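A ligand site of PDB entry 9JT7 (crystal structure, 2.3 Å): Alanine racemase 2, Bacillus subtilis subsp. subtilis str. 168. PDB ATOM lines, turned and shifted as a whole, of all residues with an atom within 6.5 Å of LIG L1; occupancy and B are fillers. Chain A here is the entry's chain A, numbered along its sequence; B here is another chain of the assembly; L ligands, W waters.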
ATOM      1  N   VAL A  41      32.182 -19.114  12.543  1.00  0.00           N
ATOM      2  CA  VAL A  41      32.460 -20.315  13.331  1.00  0.00           C
ATOM      3  C   VAL A  41      32.083 -21.575  12.532  1.00  0.00           C
ATOM      4  O   VAL A  41      30.898 -21.794  12.216  1.00  0.00           O
ATOM      5  CB  VAL A  41      31.705 -20.275  14.682  1.00  0.00           C
ATOM      6  CG1 VAL A  41      32.160 -21.419  15.615  1.00  0.00           C
ATOM      7  CG2 VAL A  41      31.905 -18.913  15.345  1.00  0.00           C
ATOM      8  N   LYS A  43      33.429 -24.971  13.278  1.00  0.00           N
ATOM      9  CA  LYS A  43      33.837 -26.161  13.978  1.00  0.00           C
ATOM     10  C   LYS A  43      32.799 -27.292  13.788  1.00  0.00           C
ATOM     11  O   LYS A  43      31.688 -27.072  13.274  1.00  0.00           O
ATOM     12  CB  LYS A  43      34.018 -25.853  15.462  1.00  0.00           C
ATOM     13  CG  LYS A  43      32.709 -25.624  16.186  1.00  0.00           C
ATOM     14  CD  LYS A  43      32.885 -24.877  17.494  1.00  0.00           C
ATOM     15  CE  LYS A  43      31.583 -24.896  18.296  1.00  0.00           C
ATOM     16  NZ  LYS A  43      31.752 -24.436  19.690  1.00  0.00           N
ATOM     17  N   TYR A  47      29.085 -27.363  11.574  1.00  0.00           N
ATOM     18  CA  TYR A  47      27.830 -27.756  12.251  1.00  0.00           C
ATOM     19  C   TYR A  47      27.080 -28.844  11.464  1.00  0.00           C
ATOM     20  O   TYR A  47      25.845 -28.838  11.373  1.00  0.00           O
ATOM     21  CB  TYR A  47      26.913 -26.551  12.499  1.00  0.00           C
ATOM     22  CG  TYR A  47      27.332 -25.556  13.588  1.00  0.00           C
ATOM     23  CD1 TYR A  47      28.666 -25.396  13.966  1.00  0.00           C
ATOM     24  CD2 TYR A  47      26.387 -24.737  14.206  1.00  0.00           C
ATOM     25  CE1 TYR A  47      29.058 -24.455  14.949  1.00  0.00           C
ATOM     26  CE2 TYR A  47      26.752 -23.786  15.200  1.00  0.00           C
ATOM     27  CZ  TYR A  47      28.086 -23.656  15.568  1.00  0.00           C
ATOM     28  OH  TYR A  47      28.431 -22.724  16.532  1.00  0.00           O
ATOM     29  N   LEU A  89      39.284 -22.512  19.737  1.00  0.00           N
ATOM     30  CA  LEU A  89      38.454 -22.082  20.856  1.00  0.00           C
ATOM     31  C   LEU A  89      38.621 -22.931  22.114  1.00  0.00           C
ATOM     32  O   LEU A  89      38.373 -22.423  23.221  1.00  0.00           O
ATOM     33  CB  LEU A  89      36.986 -22.098  20.435  1.00  0.00           C
ATOM     34  CG  LEU A  89      36.559 -20.873  19.627  1.00  0.00           C
ATOM     35  CD1 LEU A  89      35.095 -21.002  19.223  1.00  0.00           C
ATOM     36  CD2 LEU A  89      36.781 -19.604  20.453  1.00  0.00           C
ATOM     37  N   ARG A 143      33.847 -22.482  32.226  1.00  0.00           N
ATOM     38  CA  ARG A 143      34.391 -23.575  31.441  1.00  0.00           C
ATOM     39  C   ARG A 143      35.916 -23.460  31.351  1.00  0.00           C
ATOM     40  O   ARG A 143      36.626 -24.277  31.954  1.00  0.00           O
ATOM     41  CB  ARG A 143      33.748 -23.588  30.051  1.00  0.00           C
ATOM     42  CG  ARG A 143      34.216 -24.711  29.057  1.00  0.00           C
ATOM     43  CD  ARG A 143      33.263 -24.834  27.827  1.00  0.00           C
ATOM     44  NE  ARG A 143      33.079 -23.557  27.106  1.00  0.00           N
ATOM     45  CZ  ARG A 143      32.287 -23.389  26.063  1.00  0.00           C
ATOM     46  NH1 ARG A 143      31.571 -24.385  25.563  1.00  0.00           N
ATOM     47  NH2 ARG A 143      32.204 -22.180  25.502  1.00  0.00           N
ATOM     48  N   PHE A 171      38.949 -12.109  24.876  1.00  0.00           N
ATOM     49  CA  PHE A 171      37.512 -12.333  24.719  1.00  0.00           C
ATOM     50  C   PHE A 171      36.888 -12.931  25.976  1.00  0.00           C
ATOM     51  O   PHE A 171      37.585 -13.279  26.939  1.00  0.00           O
ATOM     52  CB  PHE A 171      37.216 -13.222  23.510  1.00  0.00           C
ATOM     53  CG  PHE A 171      37.720 -14.648  23.618  1.00  0.00           C
ATOM     54  CD1 PHE A 171      39.051 -14.958  23.357  1.00  0.00           C
ATOM     55  CD2 PHE A 171      36.857 -15.685  23.901  1.00  0.00           C
ATOM     56  CE1 PHE A 171      39.507 -16.275  23.410  1.00  0.00           C
ATOM     57  CE2 PHE A 171      37.303 -17.004  23.952  1.00  0.00           C
ATOM     58  CZ  PHE A 171      38.628 -17.299  23.706  1.00  0.00           C
ATOM     59  N   THR A 172      35.566 -13.074  25.933  1.00  0.00           N
ATOM     60  CA  THR A 172      34.757 -13.722  26.971  1.00  0.00           C
ATOM     61  C   THR A 172      33.563 -14.393  26.287  1.00  0.00           C
ATOM     62  O   THR A 172      33.366 -14.270  25.067  1.00  0.00           O
ATOM     63  CB  THR A 172      34.334 -12.702  28.032  1.00  0.00           C
ATOM     64  OG1 THR A 172      33.913 -13.381  29.223  1.00  0.00           O
ATOM     65  CG2 THR A 172      33.188 -11.776  27.519  1.00  0.00           C
ATOM     66  N   HIS A 173      32.737 -15.104  27.071  1.00  0.00           N
ATOM     67  CA  HIS A 173      31.561 -15.801  26.539  1.00  0.00           C
ATOM     68  C   HIS A 173      30.348 -15.700  27.476  1.00  0.00           C
ATOM     69  O   HIS A 173      30.457 -15.954  28.676  1.00  0.00           O
ATOM     70  CB  HIS A 173      31.914 -17.268  26.246  1.00  0.00           C
ATOM     71  CG  HIS A 173      30.977 -17.939  25.275  1.00  0.00           C
ATOM     72  ND1 HIS A 173      30.776 -17.462  23.988  1.00  0.00           N
ATOM     73  CD2 HIS A 173      30.181 -19.029  25.401  1.00  0.00           C
ATOM     74  CE1 HIS A 173      29.881 -18.210  23.378  1.00  0.00           C
ATOM     75  NE2 HIS A 173      29.513 -19.182  24.206  1.00  0.00           N
ATOM     76  N   CYS A 212      30.551 -11.168  21.633  1.00  0.00           N
ATOM     77  CA  CYS A 212      29.196 -11.575  21.258  1.00  0.00           C
ATOM     78  C   CYS A 212      29.165 -12.898  20.490  1.00  0.00           C
ATOM     79  O   CYS A 212      30.091 -13.220  19.745  1.00  0.00           O
ATOM     80  CB  CYS A 212      28.551 -10.502  20.365  1.00  0.00           C
ATOM     81  SG  CYS A 212      28.040  -8.934  21.159  1.00  0.00           S
ATOM     82  N   ASN A 213      28.052 -13.641  20.649  1.00  0.00           N
ATOM     83  CA  ASN A 213      27.642 -14.778  19.801  1.00  0.00           C
ATOM     84  C   ASN A 213      26.393 -14.366  18.994  1.00  0.00           C
ATOM     85  O   ASN A 213      25.965 -13.203  19.054  1.00  0.00           O
ATOM     86  CB  ASN A 213      27.419 -16.048  20.656  1.00  0.00           C
ATOM     87  CG  ASN A 213      26.362 -15.871  21.762  1.00  0.00           C
ATOM     88  OD1 ASN A 213      25.688 -14.820  21.831  1.00  0.00           O
ATOM     89  ND2 ASN A 213      26.205 -16.872  22.626  1.00  0.00           N
ATOM     90  N   THR A 214      25.799 -15.318  18.248  1.00  0.00           N
ATOM     91  CA  THR A 214      24.635 -14.998  17.400  1.00  0.00           C
ATOM     92  C   THR A 214      23.536 -14.286  18.187  1.00  0.00           C
ATOM     93  O   THR A 214      23.019 -13.249  17.752  1.00  0.00           O
ATOM     94  CB  THR A 214      24.065 -16.269  16.733  1.00  0.00           C
ATOM     95  OG1 THR A 214      25.066 -16.939  15.959  1.00  0.00           O
ATOM     96  CG2 THR A 214      22.882 -15.929  15.795  1.00  0.00           C
ATOM     97  N   ALA A 215      23.160 -14.834  19.351  1.00  0.00           N
ATOM     98  CA  ALA A 215      22.090 -14.248  20.154  1.00  0.00           C
ATOM     99  C   ALA A 215      22.510 -12.901  20.732  1.00  0.00           C
ATOM    100  O   ALA A 215      21.713 -11.955  20.764  1.00  0.00           O
ATOM    101  CB  ALA A 215      21.674 -15.192  21.292  1.00  0.00           C
ATOM    102  N   ARG A 229      31.394 -13.243  16.846  1.00  0.00           N
ATOM    103  CA  ARG A 229      31.536 -14.640  16.413  1.00  0.00           C
ATOM    104  C   ARG A 229      30.171 -15.194  16.011  1.00  0.00           C
ATOM    105  O   ARG A 229      29.359 -15.563  16.864  1.00  0.00           O
ATOM    106  CB  ARG A 229      32.199 -15.492  17.506  1.00  0.00           C
ATOM    107  CG  ARG A 229      33.512 -14.885  18.047  1.00  0.00           C
ATOM    108  CD  ARG A 229      34.195 -15.721  19.179  1.00  0.00           C
ATOM    109  NE  ARG A 229      33.322 -15.965  20.330  1.00  0.00           N
ATOM    110  CZ  ARG A 229      33.267 -15.220  21.430  1.00  0.00           C
ATOM    111  NH1 ARG A 229      34.007 -14.129  21.583  1.00  0.00           N
ATOM    112  NH2 ARG A 229      32.460 -15.593  22.420  1.00  0.00           N
ATOM    113  N   LEU A 230      29.929 -15.279  14.707  1.00  0.00           N
ATOM    114  CA  LEU A 230      28.650 -15.716  14.142  1.00  0.00           C
ATOM    115  C   LEU A 230      28.690 -17.226  13.840  1.00  0.00           C
ATOM    116  O   LEU A 230      29.455 -17.655  12.988  1.00  0.00           O
ATOM    117  CB  LEU A 230      28.370 -14.912  12.877  1.00  0.00           C
ATOM    118  CG  LEU A 230      27.113 -15.133  12.035  1.00  0.00           C
ATOM    119  CD1 LEU A 230      25.911 -14.459  12.649  1.00  0.00           C
ATOM    120  CD2 LEU A 230      27.326 -14.594  10.647  1.00  0.00           C
ATOM    121  N   GLY A 231      27.847 -18.002  14.527  1.00  0.00           N
ATOM    122  CA  GLY A 231      27.796 -19.453  14.339  1.00  0.00           C
ATOM    123  C   GLY A 231      26.481 -19.987  13.769  1.00  0.00           C
ATOM    124  O   GLY A 231      26.305 -20.032  12.550  1.00  0.00           O
ATOM    125  N   ILE A 232      25.538 -20.361  14.648  1.00  0.00           N
ATOM    126  CA  ILE A 232      24.262 -20.975  14.248  1.00  0.00           C
ATOM    127  C   ILE A 232      23.471 -20.089  13.277  1.00  0.00           C
ATOM    128  O   ILE A 232      22.696 -20.610  12.458  1.00  0.00           O
ATOM    129  CB  ILE A 232      23.425 -21.328  15.516  1.00  0.00           C
ATOM    130  CG1 ILE A 232      22.216 -22.209  15.174  1.00  0.00           C
ATOM    131  CG2 ILE A 232      22.927 -20.056  16.258  1.00  0.00           C
ATOM    132  CD1 ILE A 232      22.590 -23.684  14.891  1.00  0.00           C
ATOM    133  N   GLY A 233      23.616 -18.766  13.371  1.00  0.00           N
ATOM    134  CA  GLY A 233      22.923 -17.880  12.433  1.00  0.00           C
ATOM    135  C   GLY A 233      23.428 -17.957  11.009  1.00  0.00           C
ATOM    136  O   GLY A 233      22.678 -17.666  10.074  1.00  0.00           O
ATOM    137  N   PRO A 239      18.960 -19.123  17.635  1.00  0.00           N
ATOM    138  CA  PRO A 239      19.463 -19.695  18.905  1.00  0.00           C
ATOM    139  C   PRO A 239      18.381 -20.239  19.808  1.00  0.00           C
ATOM    140  O   PRO A 239      18.593 -21.252  20.469  1.00  0.00           O
ATOM    141  CB  PRO A 239      20.202 -18.512  19.574  1.00  0.00           C
ATOM    142  CG  PRO A 239      20.222 -17.392  18.563  1.00  0.00           C
ATOM    143  CD  PRO A 239      19.607 -17.852  17.285  1.00  0.00           C
ATOM    144  N   TYR A 368      20.870 -27.330  17.247  1.00  0.00           N
ATOM    145  CA  TYR A 368      22.309 -27.574  17.253  1.00  0.00           C
ATOM    146  C   TYR A 368      22.675 -29.056  17.178  1.00  0.00           C
ATOM    147  O   TYR A 368      23.599 -29.429  16.458  1.00  0.00           O
ATOM    148  CB  TYR A 368      22.960 -27.002  18.518  1.00  0.00           C
ATOM    149  CG  TYR A 368      23.033 -25.482  18.720  1.00  0.00           C
ATOM    150  CD1 TYR A 368      21.920 -24.751  19.078  1.00  0.00           C
ATOM    151  CD2 TYR A 368      24.250 -24.788  18.579  1.00  0.00           C
ATOM    152  CE1 TYR A 368      21.997 -23.347  19.306  1.00  0.00           C
ATOM    153  CE2 TYR A 368      24.346 -23.403  18.782  1.00  0.00           C
ATOM    154  CZ  TYR A 368      23.212 -22.682  19.156  1.00  0.00           C
ATOM    155  OH  TYR A 368      23.296 -21.309  19.386  1.00  0.00           O
ATOM    156  N   TYR B 276      25.794 -23.431  30.012  1.00  0.00           N
ATOM    157  CA  TYR B 276      24.661 -22.710  29.434  1.00  0.00           C
ATOM    158  C   TYR B 276      23.398 -22.941  30.258  1.00  0.00           C
ATOM    159  O   TYR B 276      23.146 -24.036  30.774  1.00  0.00           O
ATOM    160  CB  TYR B 276      24.350 -23.159  27.995  1.00  0.00           C
ATOM    161  CG  TYR B 276      25.402 -22.832  26.945  1.00  0.00           C
ATOM    162  CD1 TYR B 276      25.671 -21.527  26.551  1.00  0.00           C
ATOM    163  CD2 TYR B 276      26.110 -23.864  26.315  1.00  0.00           C
ATOM    164  CE1 TYR B 276      26.650 -21.254  25.570  1.00  0.00           C
ATOM    165  CE2 TYR B 276      27.077 -23.600  25.351  1.00  0.00           C
ATOM    166  CZ  TYR B 276      27.342 -22.304  24.986  1.00  0.00           C
ATOM    167  OH  TYR B 276      28.302 -22.097  24.023  1.00  0.00           O
ATOM    168  N   MET B 324      28.761 -28.523  22.759  1.00  0.00           N
ATOM    169  CA  MET B 324      29.090 -29.177  21.487  1.00  0.00           C
ATOM    170  C   MET B 324      30.433 -29.917  21.566  1.00  0.00           C
ATOM    171  O   MET B 324      30.552 -31.033  21.040  1.00  0.00           O
ATOM    172  CB  MET B 324      29.087 -28.130  20.365  1.00  0.00           C
ATOM    173  CG  MET B 324      29.600 -28.585  19.021  1.00  0.00           C
ATOM    174  SD  MET B 324      28.978 -27.647  17.559  1.00  0.00           S
ATOM    175  CE  MET B 324      27.367 -27.063  18.075  1.00  0.00           C
ATOM    176  N   ASP B 325      31.427 -29.317  22.235  1.00  0.00           N
ATOM    177  CA  ASP B 325      32.805 -29.823  22.256  1.00  0.00           C
ATOM    178  C   ASP B 325      33.332 -30.171  23.643  1.00  0.00           C
ATOM    179  O   ASP B 325      34.412 -30.788  23.719  1.00  0.00           O
ATOM    180  CB  ASP B 325      33.778 -28.801  21.652  1.00  0.00           C
ATOM    181  CG  ASP B 325      33.344 -28.325  20.264  1.00  0.00           C
ATOM    182  OD1 ASP B 325      32.986 -29.175  19.420  1.00  0.00           O
ATOM    183  OD2 ASP B 325      33.375 -27.101  20.006  1.00  0.00           O
ATOM    184  N   MET B 326      32.634 -29.821  24.731  1.00  0.00           N
ATOM    185  CA  MET B 326      33.176 -29.992  26.082  1.00  0.00           C
ATOM    186  C   MET B 326      32.068 -30.312  27.085  1.00  0.00           C
ATOM    187  O   MET B 326      30.900 -29.946  26.876  1.00  0.00           O
ATOM    188  CB  MET B 326      33.910 -28.723  26.556  1.00  0.00           C
ATOM    189  CG  MET B 326      35.157 -28.361  25.751  1.00  0.00           C
ATOM    190  SD  MET B 326      35.941 -26.858  26.412  1.00  0.00           S
ATOM    191  CE  MET B 326      35.503 -25.675  25.134  1.00  0.00           C
HETATM  192  N1  LIG L   1      31.723 -18.287  20.536  1.00  0.00           N
HETATM  193  C1  LIG L   1      32.023 -19.330  21.324  1.00  0.00           C
HETATM  194  C2  LIG L   1      33.060 -19.175  22.458  1.00  0.00           C
HETATM  195  C3  LIG L   1      31.385 -20.557  21.150  1.00  0.00           C
HETATM  196  O1  LIG L   1      31.674 -21.669  21.978  1.00  0.00           O
HETATM  197  C4  LIG L   1      30.456 -20.644  20.125  1.00  0.00           C
HETATM  198  C5  LIG L   1      29.739 -21.966  19.890  1.00  0.00           C
HETATM  199  C6  LIG L   1      30.185 -19.530  19.310  1.00  0.00           C
HETATM  200  C7  LIG L   1      30.840 -18.338  19.549  1.00  0.00           C
HETATM  201  C8  LIG L   1      29.139 -19.631  18.203  1.00  0.00           C
HETATM  202  O2  LIG L   1      27.981 -19.855  18.967  1.00  0.00           O
HETATM  203  P1  LIG L   1      26.505 -19.700  18.315  1.00  0.00           P
HETATM  204  O3  LIG L   1      25.454 -19.791  19.420  1.00  0.00           O
HETATM  205  O4  LIG L   1      26.331 -20.850  17.354  1.00  0.00           O
HETATM  206  O5  LIG L   1      26.455 -18.382  17.602  1.00  0.00           O
HETATM  207  N1  LG2 L   2      26.749 -25.695  22.809  1.00  0.00           N
HETATM  208  C1  LG2 L   2      27.635 -25.198  21.741  1.00  0.00           C
HETATM  209  C2  LG2 L   2      29.039 -25.116  22.239  1.00  0.00           C
HETATM  210  O1  LG2 L   2      29.558 -26.045  22.836  1.00  0.00           O
HETATM  211  C3  LG2 L   2      27.169 -23.807  21.225  1.00  0.00           C
HETATM  212  O2  LG2 L   2      29.744 -24.140  22.034  1.00  0.00           O
HETATM  213  O   HOH W   1      23.893 -17.719  20.295  1.00  0.00           O
HETATM  214  O   HOH W   2      33.852 -23.178  22.552  1.00  0.00           O
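N of Gly 231 sits at hydrogen-bond distance from OG1 of Thr 214, at 3.3 Å.
The side-chain hydroxyl (OG1) of Thr 214 sits at hydrogen-bond distance from the backbone NH (N) of Gly 233, at 3.5 Å.
The guanidinium group (NH2) of Arg 229 is in hydrogen-bond range of a ring nitrogen (ND1) of His 173 (3.0 Å).
O of Cys 212 is in hydrogen-bond range of N of Arg 229 (3.2 Å).
O of Thr 172 sits at hydrogen-bond distance from NH2 of Arg 229 (3.1 Å).
NE2 of His 173 sits at hydrogen-bond distance from OH of Tyr 276 of chain B (3.2 Å).
NZ of Lys 43 is in salt-bridge range of OD2 of Asp 325 of chain B.
O5 of LIG L1 lies within hydrogen-bond range of N of Thr 214 (3.2 Å).
O5 of LIG L1 sits at hydrogen-bond distance from OG1 of Thr 214 (2.6 Å).
OH of Tyr 368 lies within hydrogen-bond range of O3 of LIG L1 (2.6 Å).
NE of Arg 229 sits at hydrogen-bond distance from N1 of LIG L1.
The backbone NH of Ile 232 is in hydrogen-bond range of an oxygen (O4) of LIG L1 (2.9 Å).
OH of Tyr 47 lies within hydrogen-bond range of O4 of LIG L1 (2.9 Å).
The backbone NH of Gly 231 sits at hydrogen-bond distance from an oxygen (O5) of LIG L1, 3.4 Å away.
NZ of Lys 43 lies within salt-bridge range of O2 of LG2 L2.
The guanidinium group (NH1) of Arg 143 lies within salt-bridge range of an oxygen (O1) of LG2 L2, at 3.8 Å.
O2 of LG2 L2 lies within hydrogen-bond range of OH of Tyr 276 of chain B (3.2 Å).
N of Met 324 of chain B is in hydrogen-bond range of O1 of LG2 L2, 2.6 Å away.
An oxygen (O2) of LG2 L2 sits close to an oxygen (O1) of LIG L1 (3.1 Å).
NZ of Lys 43 touches C5 of LIG L1 (3.2 Å).
Arg 143 touches LIG L1 (NH2 to O1, 3.6 Å).
CE1 of His 173 touches C1 of LIG L1 (3.2 Å).
Asn 213 touches LIG L1.
Tyr 276 of chain B touches LIG L1.
Hydrophobic or aromatic side chains that line LIG L1: Tyr 47, His 173, Ile 232 and Tyr 368.
Of the 23 residues printed, 11 come within 4 Å of LIG L1.
The nearest printed residue that does not touch LIG L1 is Val 41 (4.04 Å).
Water W1 lies within hydrogen-bond range of O3 of LIG L1 (2.7 Å), N of Ala 215 (3.1 Å) and ND2 of Asn 213 (3.4 Å).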
